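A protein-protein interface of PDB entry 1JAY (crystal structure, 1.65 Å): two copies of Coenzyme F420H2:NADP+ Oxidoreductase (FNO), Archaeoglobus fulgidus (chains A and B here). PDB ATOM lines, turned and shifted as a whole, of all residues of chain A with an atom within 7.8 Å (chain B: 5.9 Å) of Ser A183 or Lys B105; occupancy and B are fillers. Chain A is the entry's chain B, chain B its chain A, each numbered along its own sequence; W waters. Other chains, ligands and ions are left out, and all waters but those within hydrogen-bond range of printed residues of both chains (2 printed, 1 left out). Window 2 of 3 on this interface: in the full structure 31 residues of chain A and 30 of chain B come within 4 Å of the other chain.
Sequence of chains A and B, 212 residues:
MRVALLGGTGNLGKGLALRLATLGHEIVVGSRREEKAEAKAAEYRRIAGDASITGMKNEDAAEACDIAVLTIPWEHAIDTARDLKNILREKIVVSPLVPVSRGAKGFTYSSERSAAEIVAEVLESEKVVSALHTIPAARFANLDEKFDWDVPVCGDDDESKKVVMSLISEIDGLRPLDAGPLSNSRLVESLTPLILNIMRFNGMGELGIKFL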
ATOM      1  N   ARG A 113      28.389  -4.685  21.019  1.00  0.00           N
ATOM      2  CA  ARG A 113      27.249  -3.783  21.102  1.00  0.00           C
ATOM      3  C   ARG A 113      27.584  -2.753  22.180  1.00  0.00           C
ATOM      4  O   ARG A 113      28.279  -3.073  23.148  1.00  0.00           O
ATOM      5  CB  ARG A 113      25.992  -4.557  21.497  1.00  0.00           C
ATOM      6  CG  ARG A 113      24.696  -3.843  21.173  1.00  0.00           C
ATOM      7  CD  ARG A 113      23.548  -4.846  20.976  1.00  0.00           C
ATOM      8  NE  ARG A 113      22.303  -4.172  20.604  1.00  0.00           N
ATOM      9  CZ  ARG A 113      22.069  -3.618  19.418  1.00  0.00           C
ATOM     10  NH1 ARG A 113      22.992  -3.659  18.466  1.00  0.00           N
ATOM     11  NH2 ARG A 113      20.913  -2.996  19.191  1.00  0.00           N
ATOM     12  N   SER A 114      27.089  -1.539  22.027  1.00  0.00           N
ATOM     13  CA  SER A 114      27.401  -0.497  23.013  1.00  0.00           C
ATOM     14  C   SER A 114      26.789  -0.851  24.361  1.00  0.00           C
ATOM     15  O   SER A 114      25.761  -1.539  24.445  1.00  0.00           O
ATOM     16  CB  SER A 114      26.867   0.885  22.577  1.00  0.00           C
ATOM     17  OG  SER A 114      25.450   0.961  22.680  1.00  0.00           O
ATOM     18  N   ALA A 116      25.269   1.173  26.355  1.00  0.00           N
ATOM     19  CA  ALA A 116      23.950   1.810  26.469  1.00  0.00           C
ATOM     20  C   ALA A 116      22.843   0.982  25.800  1.00  0.00           C
ATOM     21  O   ALA A 116      21.747   0.834  26.342  1.00  0.00           O
ATOM     22  CB  ALA A 116      24.000   3.228  25.875  1.00  0.00           C
ATOM     23  N   GLU A 117      23.125   0.425  24.626  1.00  0.00           N
ATOM     24  CA  GLU A 117      22.124  -0.383  23.950  1.00  0.00           C
ATOM     25  C   GLU A 117      21.848  -1.669  24.719  1.00  0.00           C
ATOM     26  O   GLU A 117      20.712  -2.138  24.749  1.00  0.00           O
ATOM     27  CB  GLU A 117      22.585  -0.683  22.528  1.00  0.00           C
ATOM     28  CG  GLU A 117      22.354   0.500  21.637  1.00  0.00           C
ATOM     29  CD  GLU A 117      23.047   0.333  20.309  1.00  0.00           C
ATOM     30  OE1 GLU A 117      22.343   0.362  19.275  1.00  0.00           O
ATOM     31  OE2 GLU A 117      24.287   0.165  20.317  1.00  0.00           O
ATOM     32  N   CYS A 154      23.283  10.579  23.380  1.00  0.00           N
ATOM     33  CA  CYS A 154      22.513   9.729  22.451  1.00  0.00           C
ATOM     34  C   CYS A 154      21.276   9.178  23.108  1.00  0.00           C
ATOM     35  O   CYS A 154      21.246   8.994  24.332  1.00  0.00           O
ATOM     36  CB  CYS A 154      23.318   8.503  22.003  1.00  0.00           C
ATOM     37  SG  CYS A 154      24.793   8.835  21.071  1.00  0.00           S
ATOM     38  N   GLY A 155      20.241   8.907  22.309  1.00  0.00           N
ATOM     39  CA  GLY A 155      19.049   8.290  22.876  1.00  0.00           C
ATOM     40  C   GLY A 155      17.952   8.249  21.821  1.00  0.00           C
ATOM     41  O   GLY A 155      17.976   9.042  20.866  1.00  0.00           O
ATOM     42  N   ASP A 156      17.001   7.336  21.987  1.00  0.00           N
ATOM     43  CA  ASP A 156      15.895   7.198  21.034  1.00  0.00           C
ATOM     44  C   ASP A 156      14.631   7.909  21.465  1.00  0.00           C
ATOM     45  O   ASP A 156      13.703   8.058  20.658  1.00  0.00           O
ATOM     46  CB  ASP A 156      15.578   5.728  20.786  1.00  0.00           C
ATOM     47  CG  ASP A 156      16.764   4.969  20.226  1.00  0.00           C
ATOM     48  OD1 ASP A 156      17.538   5.582  19.466  1.00  0.00           O
ATOM     49  OD2 ASP A 156      16.917   3.773  20.537  1.00  0.00           O
ATOM     50  N   ALA A 179      24.083  13.522  19.753  1.00  0.00           N
ATOM     51  CA  ALA A 179      24.861  12.667  18.843  1.00  0.00           C
ATOM     52  C   ALA A 179      23.935  11.683  18.118  1.00  0.00           C
ATOM     53  O   ALA A 179      24.412  10.750  17.458  1.00  0.00           O
ATOM     54  CB  ALA A 179      25.979  11.910  19.585  1.00  0.00           C
ATOM     55  N   GLY A 180      22.622  11.893  18.264  1.00  0.00           N
ATOM     56  CA  GLY A 180      21.637  11.079  17.555  1.00  0.00           C
ATOM     57  C   GLY A 180      21.002   9.940  18.328  1.00  0.00           C
ATOM     58  O   GLY A 180      20.927   9.970  19.555  1.00  0.00           O
ATOM     59  N   PRO A 181      20.538   8.901  17.621  1.00  0.00           N
ATOM     60  CA  PRO A 181      19.902   7.745  18.261  1.00  0.00           C
ATOM     61  C   PRO A 181      20.872   6.940  19.122  1.00  0.00           C
ATOM     62  O   PRO A 181      22.087   7.064  18.986  1.00  0.00           O
ATOM     63  CB  PRO A 181      19.404   6.916  17.073  1.00  0.00           C
ATOM     64  CG  PRO A 181      19.224   7.939  15.970  1.00  0.00           C
ATOM     65  CD  PRO A 181      20.477   8.786  16.147  1.00  0.00           C
ATOM     66  N   LEU A 182      20.318   6.078  19.972  1.00  0.00           N
ATOM     67  CA  LEU A 182      21.142   5.273  20.840  1.00  0.00           C
ATOM     68  C   LEU A 182      22.092   4.393  20.011  1.00  0.00           C
ATOM     69  O   LEU A 182      23.134   3.982  20.513  1.00  0.00           O
ATOM     70  CB  LEU A 182      20.257   4.420  21.776  1.00  0.00           C
ATOM     71  CG  LEU A 182      20.898   4.006  23.104  1.00  0.00           C
ATOM     72  CD1 LEU A 182      21.187   5.245  23.961  1.00  0.00           C
ATOM     73  CD2 LEU A 182      19.964   3.054  23.844  1.00  0.00           C
ATOM     74  N   SER A 183      21.751   4.114  18.747  1.00  0.00           N
ATOM     75  CA  SER A 183      22.621   3.321  17.893  1.00  0.00           C
ATOM     76  C   SER A 183      23.991   3.977  17.632  1.00  0.00           C
ATOM     77  O   SER A 183      24.891   3.334  17.091  1.00  0.00           O
ATOM     78  CB  SER A 183      21.934   3.006  16.556  1.00  0.00           C
ATOM     79  OG  SER A 183      21.559   4.197  15.880  1.00  0.00           O
ATOM     80  N   ASN A 184      24.161   5.238  18.028  1.00  0.00           N
ATOM     81  CA  ASN A 184      25.441   5.916  17.839  1.00  0.00           C
ATOM     82  C   ASN A 184      26.256   5.899  19.140  1.00  0.00           C
ATOM     83  O   ASN A 184      27.335   6.471  19.212  1.00  0.00           O
ATOM     84  CB  ASN A 184      25.240   7.362  17.371  1.00  0.00           C
ATOM     85  CG  ASN A 184      24.769   7.437  15.916  1.00  0.00           C
ATOM     86  OD1 ASN A 184      25.129   6.582  15.099  1.00  0.00           O
ATOM     87  ND2 ASN A 184      23.981   8.467  15.584  1.00  0.00           N
ATOM     88  N   SER A 185      25.732   5.226  20.161  1.00  0.00           N
ATOM     89  CA  SER A 185      26.418   5.206  21.438  1.00  0.00           C
ATOM     90  C   SER A 185      27.791   4.555  21.387  1.00  0.00           C
ATOM     91  O   SER A 185      28.690   4.938  22.138  1.00  0.00           O
ATOM     92  CB  SER A 185      25.526   4.531  22.510  1.00  0.00           C
ATOM     93  OG  SER A 185      26.051   4.820  23.810  1.00  0.00           O
ATOM     94  N   ARG A 186      27.995   3.575  20.509  1.00  0.00           N
ATOM     95  CA  ARG A 186      29.314   2.963  20.464  1.00  0.00           C
ATOM     96  C   ARG A 186      30.392   3.990  20.071  1.00  0.00           C
ATOM     97  O   ARG A 186      31.521   3.952  20.556  1.00  0.00           O
ATOM     98  CB  ARG A 186      29.308   1.800  19.474  1.00  0.00           C
ATOM     99  CG  ARG A 186      30.566   0.956  19.482  1.00  0.00           C
ATOM    100  CD  ARG A 186      30.371  -0.151  18.437  1.00  0.00           C
ATOM    101  NE  ARG A 186      31.381  -1.205  18.439  1.00  0.00           N
ATOM    102  CZ  ARG A 186      32.686  -0.993  18.516  1.00  0.00           C
ATOM    103  NH1 ARG A 186      33.148   0.239  18.622  1.00  0.00           N
ATOM    104  NH2 ARG A 186      33.531  -2.015  18.428  1.00  0.00           N
ATOM    105  N   LEU A 187      30.049   4.911  19.180  1.00  0.00           N
ATOM    106  CA  LEU A 187      31.014   5.935  18.756  1.00  0.00           C
ATOM    107  C   LEU A 187      31.313   6.903  19.896  1.00  0.00           C
ATOM    108  O   LEU A 187      32.425   7.426  19.986  1.00  0.00           O
ATOM    109  CB  LEU A 187      30.459   6.748  17.567  1.00  0.00           C
ATOM    110  CG  LEU A 187      30.333   5.944  16.270  1.00  0.00           C
ATOM    111  CD1 LEU A 187      29.602   6.806  15.221  1.00  0.00           C
ATOM    112  CD2 LEU A 187      31.715   5.539  15.773  1.00  0.00           C
ATOM    113  N   VAL A 188      30.314   7.165  20.745  1.00  0.00           N
ATOM    114  CA  VAL A 188      30.520   8.083  21.868  1.00  0.00           C
ATOM    115  C   VAL A 188      31.339   7.386  22.968  1.00  0.00           C
ATOM    116  O   VAL A 188      32.283   7.958  23.521  1.00  0.00           O
ATOM    117  CB  VAL A 188      29.173   8.547  22.462  1.00  0.00           C
ATOM    118  CG1 VAL A 188      29.425   9.432  23.691  1.00  0.00           C
ATOM    119  CG2 VAL A 188      28.383   9.355  21.406  1.00  0.00           C
ATOM    120  N   GLY B 103      23.762   6.808   6.905  1.00  0.00           N
ATOM    121  CA  GLY B 103      22.601   5.958   7.052  1.00  0.00           C
ATOM    122  C   GLY B 103      21.441   6.782   7.573  1.00  0.00           C
ATOM    123  O   GLY B 103      21.628   7.939   7.927  1.00  0.00           O
ATOM    124  N   ALA B 104      20.252   6.204   7.622  1.00  0.00           N
ATOM    125  CA  ALA B 104      19.105   6.961   8.106  1.00  0.00           C
ATOM    126  C   ALA B 104      19.313   7.432   9.543  1.00  0.00           C
ATOM    127  O   ALA B 104      18.844   8.514   9.924  1.00  0.00           O
ATOM    128  CB  ALA B 104      17.829   6.102   8.017  1.00  0.00           C
ATOM    129  N   LYS B 105      20.018   6.636  10.338  1.00  0.00           N
ATOM    130  CA  LYS B 105      20.217   7.006  11.731  1.00  0.00           C
ATOM    131  C   LYS B 105      21.550   7.655  12.056  1.00  0.00           C
ATOM    132  O   LYS B 105      21.947   7.734  13.231  1.00  0.00           O
ATOM    133  CB  LYS B 105      19.985   5.783  12.613  1.00  0.00           C
ATOM    134  CG  LYS B 105      18.569   5.203  12.416  1.00  0.00           C
ATOM    135  CD  LYS B 105      18.354   3.914  13.205  1.00  0.00           C
ATOM    136  CE  LYS B 105      18.488   4.136  14.709  1.00  0.00           C
ATOM    137  NZ  LYS B 105      18.090   2.943  15.488  1.00  0.00           N
ATOM    138  N   GLY B 106      22.233   8.118  11.020  1.00  0.00           N
ATOM    139  CA  GLY B 106      23.508   8.778  11.211  1.00  0.00           C
ATOM    140  C   GLY B 106      24.670   8.080  10.522  1.00  0.00           C
ATOM    141  O   GLY B 106      24.510   7.068   9.841  1.00  0.00           O
ATOM    142  N   PHE B 107      25.857   8.613  10.749  1.00  0.00           N
ATOM    143  CA  PHE B 107      27.063   8.078  10.146  1.00  0.00           C
ATOM    144  C   PHE B 107      27.594   6.919  10.973  1.00  0.00           C
ATOM    145  O   PHE B 107      27.477   6.923  12.195  1.00  0.00           O
ATOM    146  CB  PHE B 107      28.088   9.188  10.056  1.00  0.00           C
ATOM    147  CG  PHE B 107      27.655  10.342   9.178  1.00  0.00           C
ATOM    148  CD1 PHE B 107      26.899  11.387   9.698  1.00  0.00           C
ATOM    149  CD2 PHE B 107      28.031  10.378   7.836  1.00  0.00           C
ATOM    150  CE1 PHE B 107      26.527  12.463   8.898  1.00  0.00           C
ATOM    151  CE2 PHE B 107      27.663  11.453   7.013  1.00  0.00           C
ATOM    152  CZ  PHE B 107      26.912  12.497   7.545  1.00  0.00           C
ATOM    153  N   ASN B 197      28.283  12.997  12.991  1.00  0.00           N
ATOM    154  CA  ASN B 197      26.987  12.891  13.671  1.00  0.00           C
ATOM    155  C   ASN B 197      26.700  14.144  14.516  1.00  0.00           C
ATOM    156  O   ASN B 197      25.568  14.629  14.557  1.00  0.00           O
ATOM    157  CB  ASN B 197      26.949  11.639  14.551  1.00  0.00           C
ATOM    158  CG  ASN B 197      26.634  10.375  13.745  1.00  0.00           C
ATOM    159  OD1 ASN B 197      25.753  10.392  12.890  1.00  0.00           O
ATOM    160  ND2 ASN B 197      27.338   9.274  14.032  1.00  0.00           N
ATOM    161  N   ARG B 200      25.614  16.791  12.144  1.00  0.00           N
ATOM    162  CA  ARG B 200      24.285  16.497  11.650  1.00  0.00           C
ATOM    163  C   ARG B 200      23.194  16.780  12.661  1.00  0.00           C
ATOM    164  O   ARG B 200      22.228  17.493  12.360  1.00  0.00           O
ATOM    165  CB  ARG B 200      24.199  15.029  11.207  1.00  0.00           C
ATOM    166  CG  ARG B 200      22.791  14.607  10.810  1.00  0.00           C
ATOM    167  CD  ARG B 200      22.742  13.220  10.174  1.00  0.00           C
ATOM    168  NE  ARG B 200      21.373  12.715  10.215  1.00  0.00           N
ATOM    169  CZ  ARG B 200      20.983  11.498   9.833  1.00  0.00           C
ATOM    170  NH1 ARG B 200      21.859  10.623   9.349  1.00  0.00           N
ATOM    171  NH2 ARG B 200      19.715  11.131   9.999  1.00  0.00           N
ATOM    172  N   PHE B 201      23.359  16.256  13.872  1.00  0.00           N
ATOM    173  CA  PHE B 201      22.316  16.404  14.877  1.00  0.00           C
ATOM    174  C   PHE B 201      22.255  17.712  15.663  1.00  0.00           C
ATOM    175  O   PHE B 201      21.297  17.925  16.413  1.00  0.00           O
ATOM    176  CB  PHE B 201      22.335  15.170  15.806  1.00  0.00           C
ATOM    177  CG  PHE B 201      21.987  13.876  15.097  1.00  0.00           C
ATOM    178  CD1 PHE B 201      22.973  12.936  14.774  1.00  0.00           C
ATOM    179  CD2 PHE B 201      20.672  13.624  14.685  1.00  0.00           C
ATOM    180  CE1 PHE B 201      22.669  11.787  14.054  1.00  0.00           C
ATOM    181  CE2 PHE B 201      20.346  12.461  13.954  1.00  0.00           C
ATOM    182  CZ  PHE B 201      21.353  11.540  13.636  1.00  0.00           C
HETATM  183  O   HOH W   1      23.435   4.654  13.799  1.00  0.00           O
HETATM  184  O   HOH W   2      27.174   4.586  14.646  1.00  0.00           O
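O of Lys B105 sits at hydrogen-bond distance from ND2 of Asn A184.
The backbone NH (N) of Phe B107 is in hydrogen-bond range of the side-chain amide oxygen (OD1) of Asn B197.
The backbone carbonyl oxygen of Ala A179 lies within hydrogen-bond range of the side-chain amide nitrogen of Asn A184 (3.0 Å).
The backbone NH (N) of Gly A155 lies within hydrogen-bond range of the backbone carbonyl oxygen (O) of Gly A180.
Among the printed residues, pairs that only touch across the chains: Ala A179 with Asn B197 (3.96 Å), Ala A179 with Phe B201 (3.7 Å), Gly A180 with Phe B201 (3.6 Å), Pro A181 with Lys B105 (3.4 Å), Pro A181 with Phe B201 (3.8 Å), Ser A183 with Lys B105 (3.3 Å), Asn A184 with Phe B107 (3.8 Å), Asn A184 with Asn B197 (3.6 Å), Asn A184 with Phe B201 (3.9 Å), Leu A187 with Phe B107 (3.7 Å) and Leu A187 with Asn B197 (3.6 Å).
Lys B105 touches just these residues of chain A: Pro A181, Ser A183 and Asn A184.
No residue of chain A comes within 4 Å of Gly B106.
Of the printed residues of chain A, Asn B197 touches Ala A179 (3.96 Å), Asn A184 (3.6 Å) and Leu A187 (3.6 Å).
Printed residues of chain B within 4 Å of Ala A179: Asn B197 and Phe B201.
Printed residues of chain B within 4 Å of Gly A180: Phe B201 (3.6 Å).
Printed residues of chain B within 4 Å of Pro A181: Lys B105 and Phe B201.
Printed residues of chain B within 4 Å of Asn A184: Lys B105, Phe B107, Asn B197 and Phe B201.
Cys A154 touches none of the printed residues of chain B.
The nearest printed residue of chain B that does not touch Ser A183 is Gly B106 (6.3 Å).
The nearest residue of chain A that does not touch Lys B105 is Asp A156 (4.8 Å).
The nearest printed residue of chain A that does not touch Phe B201 is Ser A183 (7.7 Å).
Of the 8 printed residues of chain B, 4 touch a printed residue of chain A.
Hydrophobic or aromatic side chains of chain B within 4 Å of the printed part of chain A: Phe B201.
Among the printed residues, 12 pairs touch across the chains.
Among the printed residues, no Asp or Glu carboxylate lies within 4 Å of a Lys or Arg side-chain nitrogen of the other chain.
No position is printed for both chains.
Water W1 lies within hydrogen-bond range of OG of Ser A183 (2.8 Å), OD1 of Asn A184 (2.9 Å) and O of Lys B105 (3.5 Å).
Water W2 lies within hydrogen-bond range of the side-chain amide oxygen of Asn A184 (2.9 Å) and the backbone carbonyl oxygen of Phe B107 (3.4 Å).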
